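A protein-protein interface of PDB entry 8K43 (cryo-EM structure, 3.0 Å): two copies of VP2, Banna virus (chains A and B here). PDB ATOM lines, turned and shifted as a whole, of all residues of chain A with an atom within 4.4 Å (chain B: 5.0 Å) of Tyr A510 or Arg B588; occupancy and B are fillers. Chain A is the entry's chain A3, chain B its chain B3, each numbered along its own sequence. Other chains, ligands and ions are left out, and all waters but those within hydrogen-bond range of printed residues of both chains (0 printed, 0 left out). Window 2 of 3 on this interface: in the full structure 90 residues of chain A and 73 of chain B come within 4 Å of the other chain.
The side-chain amide nitrogen (ND2) of Asn A514 is in hydrogen-bond range of the side-chain amide oxygen (OE1) of Gln B528, at 3.3 Å.
OH of Tyr A510 is in hydrogen-bond range of OG1 of Thr A500 (3.2 Å).
Among the printed residues, pairs that only touch across the chains: Leu A467 with Ser B591 (3.6 Å) and Tyr A510 with Arg B588 (3.4 Å).
Printed residues of chain B within 4 Å of Leu A467: Ser B591 (3.6 Å). Tyr A510 touches just one residue of chain B: Arg B588. Of the printed residues of chain B, Asn A514 touches Gln B528 (3.3 Å). Of the printed residues of chain A, Gln B528 touches Asn A514. Printed residues of chain A within 4 Å of Ser B591: Leu A467. The nearest printed residue of chain B that does not touch Tyr A510 is Arg B586 (8.2 Å). The nearest residue of chain A that does not touch Arg B588 is Leu A467 (4.2 Å).
Hydrophobic or aromatic side chains of chain A that line the printed part of chain B: Leu A467 and Tyr A510. Of the 10 printed residues of chain B, 3 touch a printed residue of chain A. Along chain B the printed residues that touch a printed residue of chain A span positions 528 to 591. Among the printed residues, 3 pairs touch across the chains.
No position is printed for both chains.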
ATOM      1  N   ALA A 466       7.234  17.146 -18.808  1.00  0.00           N
ATOM      2  CA  ALA A 466       6.459  17.236 -20.033  1.00  0.00           C
ATOM      3  C   ALA A 466       7.336  16.930 -21.244  1.00  0.00           C
ATOM      4  O   ALA A 466       8.564  16.873 -21.163  1.00  0.00           O
ATOM      5  CB  ALA A 466       5.828  18.621 -20.168  1.00  0.00           C
ATOM      6  N   LEU A 467       6.677  16.715 -22.384  1.00  0.00           N
ATOM      7  CA  LEU A 467       7.405  16.449 -23.620  1.00  0.00           C
ATOM      8  C   LEU A 467       8.264  17.640 -24.019  1.00  0.00           C
ATOM      9  O   LEU A 467       9.413  17.472 -24.442  1.00  0.00           O
ATOM     10  CB  LEU A 467       6.423  16.094 -24.734  1.00  0.00           C
ATOM     11  CG  LEU A 467       6.095  14.610 -24.896  1.00  0.00           C
ATOM     12  CD1 LEU A 467       5.536  14.341 -26.283  1.00  0.00           C
ATOM     13  CD2 LEU A 467       7.326  13.759 -24.640  1.00  0.00           C
ATOM     14  N   PRO A 469       9.790  20.747 -22.178  1.00  0.00           N
ATOM     15  CA  PRO A 469       9.938  21.361 -20.854  1.00  0.00           C
ATOM     16  C   PRO A 469       9.748  22.869 -20.894  1.00  0.00           C
ATOM     17  O   PRO A 469      10.118  23.540 -21.860  1.00  0.00           O
ATOM     18  CB  PRO A 469      11.370  20.992 -20.452  1.00  0.00           C
ATOM     19  CG  PRO A 469      11.701  19.801 -21.276  1.00  0.00           C
ATOM     20  CD  PRO A 469      10.994  20.004 -22.577  1.00  0.00           C
ATOM     21  N   THR A 500      16.493  17.493 -18.453  1.00  0.00           N
ATOM     22  CA  THR A 500      15.378  18.424 -18.590  1.00  0.00           C
ATOM     23  C   THR A 500      15.832  19.864 -18.397  1.00  0.00           C
ATOM     24  O   THR A 500      15.430  20.757 -19.151  1.00  0.00           O
ATOM     25  CB  THR A 500      14.277  18.072 -17.593  1.00  0.00           C
ATOM     26  OG1 THR A 500      13.761  16.770 -17.890  1.00  0.00           O
ATOM     27  CG2 THR A 500      13.149  19.084 -17.664  1.00  0.00           C
ATOM     28  N   VAL A 503      17.807  20.976 -21.417  1.00  0.00           N
ATOM     29  CA  VAL A 503      16.980  21.229 -22.594  1.00  0.00           C
ATOM     30  C   VAL A 503      16.434  22.651 -22.563  1.00  0.00           C
ATOM     31  O   VAL A 503      16.469  23.372 -23.567  1.00  0.00           O
ATOM     32  CB  VAL A 503      15.849  20.191 -22.687  1.00  0.00           C
ATOM     33  CG1 VAL A 503      14.743  20.692 -23.595  1.00  0.00           C
ATOM     34  CG2 VAL A 503      16.389  18.869 -23.196  1.00  0.00           C
ATOM     35  N   THR A 508      18.869  22.855 -25.861  1.00  0.00           N
ATOM     36  CA  THR A 508      19.251  21.758 -26.734  1.00  0.00           C
ATOM     37  C   THR A 508      18.135  20.726 -26.742  1.00  0.00           C
ATOM     38  O   THR A 508      17.317  20.675 -25.821  1.00  0.00           O
ATOM     39  CB  THR A 508      20.571  21.119 -26.284  1.00  0.00           C
ATOM     40  OG1 THR A 508      21.221  20.517 -27.409  1.00  0.00           O
ATOM     41  CG2 THR A 508      20.329  20.068 -25.214  1.00  0.00           C
ATOM     42  N   THR A 509      18.082  19.935 -27.808  1.00  0.00           N
ATOM     43  CA  THR A 509      17.046  18.928 -27.958  1.00  0.00           C
ATOM     44  C   THR A 509      17.310  17.737 -27.036  1.00  0.00           C
ATOM     45  O   THR A 509      18.436  17.497 -26.591  1.00  0.00           O
ATOM     46  CB  THR A 509      16.968  18.475 -29.414  1.00  0.00           C
ATOM     47  OG1 THR A 509      17.023  19.625 -30.263  1.00  0.00           O
ATOM     48  CG2 THR A 509      15.662  17.751 -29.685  1.00  0.00           C
ATOM     49  N   TYR A 510      16.241  16.991 -26.745  1.00  0.00           N
ATOM     50  CA  TYR A 510      16.357  15.808 -25.898  1.00  0.00           C
ATOM     51  C   TYR A 510      17.255  14.755 -26.531  1.00  0.00           C
ATOM     52  O   TYR A 510      18.019  14.078 -25.833  1.00  0.00           O
ATOM     53  CB  TYR A 510      14.972  15.224 -25.630  1.00  0.00           C
ATOM     54  CG  TYR A 510      14.321  15.700 -24.354  1.00  0.00           C
ATOM     55  CD1 TYR A 510      14.759  15.248 -23.122  1.00  0.00           C
ATOM     56  CD2 TYR A 510      13.264  16.596 -24.384  1.00  0.00           C
ATOM     57  CE1 TYR A 510      14.166  15.673 -21.957  1.00  0.00           C
ATOM     58  CE2 TYR A 510      12.666  17.029 -23.222  1.00  0.00           C
ATOM     59  CZ  TYR A 510      13.120  16.563 -22.011  1.00  0.00           C
ATOM     60  OH  TYR A 510      12.528  16.992 -20.849  1.00  0.00           O
ATOM     61  N   ASP A 511      17.166  14.589 -27.852  1.00  0.00           N
ATOM     62  CA  ASP A 511      17.964  13.571 -28.526  1.00  0.00           C
ATOM     63  C   ASP A 511      19.450  13.890 -28.472  1.00  0.00           C
ATOM     64  O   ASP A 511      20.283  12.982 -28.564  1.00  0.00           O
ATOM     65  CB  ASP A 511      17.507  13.427 -29.976  1.00  0.00           C
ATOM     66  CG  ASP A 511      16.006  13.261 -30.099  1.00  0.00           C
ATOM     67  OD1 ASP A 511      15.412  12.551 -29.260  1.00  0.00           O
ATOM     68  OD2 ASP A 511      15.420  13.845 -31.033  1.00  0.00           O
ATOM     69  N   ILE A 512      19.801  15.168 -28.326  1.00  0.00           N
ATOM     70  CA  ILE A 512      21.208  15.556 -28.288  1.00  0.00           C
ATOM     71  C   ILE A 512      21.873  15.038 -27.022  1.00  0.00           C
ATOM     72  O   ILE A 512      22.972  14.473 -27.067  1.00  0.00           O
ATOM     73  CB  ILE A 512      21.338  17.085 -28.406  1.00  0.00           C
ATOM     74  CG1 ILE A 512      21.153  17.519 -29.855  1.00  0.00           C
ATOM     75  CG2 ILE A 512      22.687  17.548 -27.890  1.00  0.00           C
ATOM     76  CD1 ILE A 512      21.921  16.678 -30.822  1.00  0.00           C
ATOM     77  N   VAL A 513      21.218  15.210 -25.876  1.00  0.00           N
ATOM     78  CA  VAL A 513      21.816  14.887 -24.588  1.00  0.00           C
ATOM     79  C   VAL A 513      21.376  13.502 -24.139  1.00  0.00           C
ATOM     80  O   VAL A 513      21.502  13.150 -22.961  1.00  0.00           O
ATOM     81  CB  VAL A 513      21.451  15.948 -23.536  1.00  0.00           C
ATOM     82  CG1 VAL A 513      22.192  17.241 -23.815  1.00  0.00           C
ATOM     83  CG2 VAL A 513      19.952  16.184 -23.526  1.00  0.00           C
ATOM     84  N   ASN A 514      20.849  12.707 -25.073  1.00  0.00           N
ATOM     85  CA  ASN A 514      20.411  11.358 -24.732  1.00  0.00           C
ATOM     86  C   ASN A 514      21.580  10.489 -24.285  1.00  0.00           C
ATOM     87  O   ASN A 514      21.470   9.745 -23.304  1.00  0.00           O
ATOM     88  CB  ASN A 514      19.699  10.718 -25.920  1.00  0.00           C
ATOM     89  CG  ASN A 514      18.884   9.507 -25.523  1.00  0.00           C
ATOM     90  OD1 ASN A 514      18.276   9.481 -24.455  1.00  0.00           O
ATOM     91  ND2 ASN A 514      18.871   8.496 -26.381  1.00  0.00           N
ATOM     92  N   PHE B 504      11.835   0.355 -31.374  1.00  0.00           N
ATOM     93  CA  PHE B 504      10.963   1.073 -30.456  1.00  0.00           C
ATOM     94  C   PHE B 504      11.743   1.851 -29.403  1.00  0.00           C
ATOM     95  O   PHE B 504      11.380   2.986 -29.075  1.00  0.00           O
ATOM     96  CB  PHE B 504      10.001   0.105 -29.776  1.00  0.00           C
ATOM     97  CG  PHE B 504       8.938   0.788 -28.983  1.00  0.00           C
ATOM     98  CD1 PHE B 504       8.075   1.678 -29.593  1.00  0.00           C
ATOM     99  CD2 PHE B 504       8.811   0.560 -27.629  1.00  0.00           C
ATOM    100  CE1 PHE B 504       7.098   2.315 -28.870  1.00  0.00           C
ATOM    101  CE2 PHE B 504       7.836   1.195 -26.903  1.00  0.00           C
ATOM    102  CZ  PHE B 504       6.979   2.075 -27.525  1.00  0.00           C
ATOM    103  N   LEU B 505      12.811   1.269 -28.863  1.00  0.00           N
ATOM    104  CA  LEU B 505      13.500   1.865 -27.725  1.00  0.00           C
ATOM    105  C   LEU B 505      14.614   2.817 -28.155  1.00  0.00           C
ATOM    106  O   LEU B 505      14.728   3.923 -27.621  1.00  0.00           O
ATOM    107  CB  LEU B 505      14.061   0.764 -26.822  1.00  0.00           C
ATOM    108  CG  LEU B 505      13.045  -0.072 -26.044  1.00  0.00           C
ATOM    109  CD1 LEU B 505      13.414  -1.544 -26.084  1.00  0.00           C
ATOM    110  CD2 LEU B 505      12.947   0.400 -24.609  1.00  0.00           C
ATOM    111  N   ASN B 507      14.879   4.326 -30.965  1.00  0.00           N
ATOM    112  CA  ASN B 507      14.339   5.320 -31.895  1.00  0.00           C
ATOM    113  C   ASN B 507      15.055   5.255 -33.246  1.00  0.00           C
ATOM    114  O   ASN B 507      15.682   6.212 -33.704  1.00  0.00           O
ATOM    115  CB  ASN B 507      14.405   6.730 -31.295  1.00  0.00           C
ATOM    116  CG  ASN B 507      13.614   7.745 -32.093  1.00  0.00           C
ATOM    117  OD1 ASN B 507      12.407   7.891 -31.911  1.00  0.00           O
ATOM    118  ND2 ASN B 507      14.297   8.461 -32.977  1.00  0.00           N
ATOM    119  N   GLN B 528      21.255   2.132 -24.204  1.00  0.00           N
ATOM    120  CA  GLN B 528      19.987   2.805 -23.962  1.00  0.00           C
ATOM    121  C   GLN B 528      19.431   2.469 -22.585  1.00  0.00           C
ATOM    122  O   GLN B 528      18.690   3.269 -22.004  1.00  0.00           O
ATOM    123  CB  GLN B 528      18.984   2.438 -25.053  1.00  0.00           C
ATOM    124  CG  GLN B 528      17.750   3.313 -25.075  1.00  0.00           C
ATOM    125  CD  GLN B 528      18.083   4.774 -25.280  1.00  0.00           C
ATOM    126  OE1 GLN B 528      18.635   5.157 -26.310  1.00  0.00           O
ATOM    127  NE2 GLN B 528      17.749   5.600 -24.298  1.00  0.00           N
ATOM    128  N   ARG B 586      14.875   5.741 -18.362  1.00  0.00           N
ATOM    129  CA  ARG B 586      13.970   6.521 -19.196  1.00  0.00           C
ATOM    130  C   ARG B 586      14.300   6.250 -20.656  1.00  0.00           C
ATOM    131  O   ARG B 586      15.444   6.440 -21.082  1.00  0.00           O
ATOM    132  CB  ARG B 586      14.079   8.016 -18.891  1.00  0.00           C
ATOM    133  CG  ARG B 586      14.327   8.348 -17.428  1.00  0.00           C
ATOM    134  CD  ARG B 586      13.223   7.810 -16.536  1.00  0.00           C
ATOM    135  NE  ARG B 586      11.992   8.583 -16.635  1.00  0.00           N
ATOM    136  CZ  ARG B 586      11.476   9.294 -15.642  1.00  0.00           C
ATOM    137  NH1 ARG B 586      12.070   9.365 -14.464  1.00  0.00           N
ATOM    138  NH2 ARG B 586      10.336   9.948 -15.838  1.00  0.00           N
ATOM    139  N   PHE B 587      13.302   5.808 -21.413  1.00  0.00           N
ATOM    140  CA  PHE B 587      13.443   5.536 -22.836  1.00  0.00           C
ATOM    141  C   PHE B 587      12.538   6.489 -23.600  1.00  0.00           C
ATOM    142  O   PHE B 587      11.408   6.748 -23.177  1.00  0.00           O
ATOM    143  CB  PHE B 587      13.076   4.089 -23.170  1.00  0.00           C
ATOM    144  CG  PHE B 587      13.853   3.068 -22.395  1.00  0.00           C
ATOM    145  CD1 PHE B 587      15.055   2.582 -22.874  1.00  0.00           C
ATOM    146  CD2 PHE B 587      13.373   2.583 -21.193  1.00  0.00           C
ATOM    147  CE1 PHE B 587      15.769   1.639 -22.164  1.00  0.00           C
ATOM    148  CE2 PHE B 587      14.079   1.642 -20.478  1.00  0.00           C
ATOM    149  CZ  PHE B 587      15.278   1.170 -20.964  1.00  0.00           C
ATOM    150  N   ARG B 588      13.033   7.016 -24.716  1.00  0.00           N
ATOM    151  CA  ARG B 588      12.246   7.927 -25.546  1.00  0.00           C
ATOM    152  C   ARG B 588      11.642   7.110 -26.681  1.00  0.00           C
ATOM    153  O   ARG B 588      12.183   7.044 -27.785  1.00  0.00           O
ATOM    154  CB  ARG B 588      13.104   9.075 -26.055  1.00  0.00           C
ATOM    155  CG  ARG B 588      13.374  10.144 -25.008  1.00  0.00           C
ATOM    156  CD  ARG B 588      12.098  10.875 -24.628  1.00  0.00           C
ATOM    157  NE  ARG B 588      11.564  11.650 -25.739  1.00  0.00           N
ATOM    158  CZ  ARG B 588      11.361  12.959 -25.712  1.00  0.00           C
ATOM    159  NH1 ARG B 588      11.633  13.676 -24.634  1.00  0.00           N
ATOM    160  NH2 ARG B 588      10.872  13.565 -26.790  1.00  0.00           N
ATOM    161  N   ASN B 589      10.505   6.482 -26.401  1.00  0.00           N
ATOM    162  CA  ASN B 589       9.844   5.573 -27.330  1.00  0.00           C
ATOM    163  C   ASN B 589       8.561   6.229 -27.822  1.00  0.00           C
ATOM    164  O   ASN B 589       7.566   6.275 -27.091  1.00  0.00           O
ATOM    165  CB  ASN B 589       9.541   4.238 -26.657  1.00  0.00           C
ATOM    166  CG  ASN B 589      10.774   3.585 -26.077  1.00  0.00           C
ATOM    167  OD1 ASN B 589      11.870   4.139 -26.132  1.00  0.00           O
ATOM    168  ND2 ASN B 589      10.600   2.398 -25.511  1.00  0.00           N
ATOM    169  N   ALA B 590       8.588   6.724 -29.060  1.00  0.00           N
ATOM    170  CA  ALA B 590       7.440   7.407 -29.661  1.00  0.00           C
ATOM    171  C   ALA B 590       6.950   8.545 -28.770  1.00  0.00           C
ATOM    172  O   ALA B 590       5.749   8.805 -28.659  1.00  0.00           O
ATOM    173  CB  ALA B 590       6.310   6.422 -29.966  1.00  0.00           C
ATOM    174  N   SER B 591       7.900   9.232 -28.132  1.00  0.00           N
ATOM    175  CA  SER B 591       7.611  10.342 -27.224  1.00  0.00           C
ATOM    176  C   SER B 591       6.643   9.927 -26.116  1.00  0.00           C
ATOM    177  O   SER B 591       5.706  10.652 -25.781  1.00  0.00           O
ATOM    178  CB  SER B 591       7.076  11.556 -27.985  1.00  0.00           C
ATOM    179  OG  SER B 591       5.718  11.374 -28.343  1.00  0.00           O
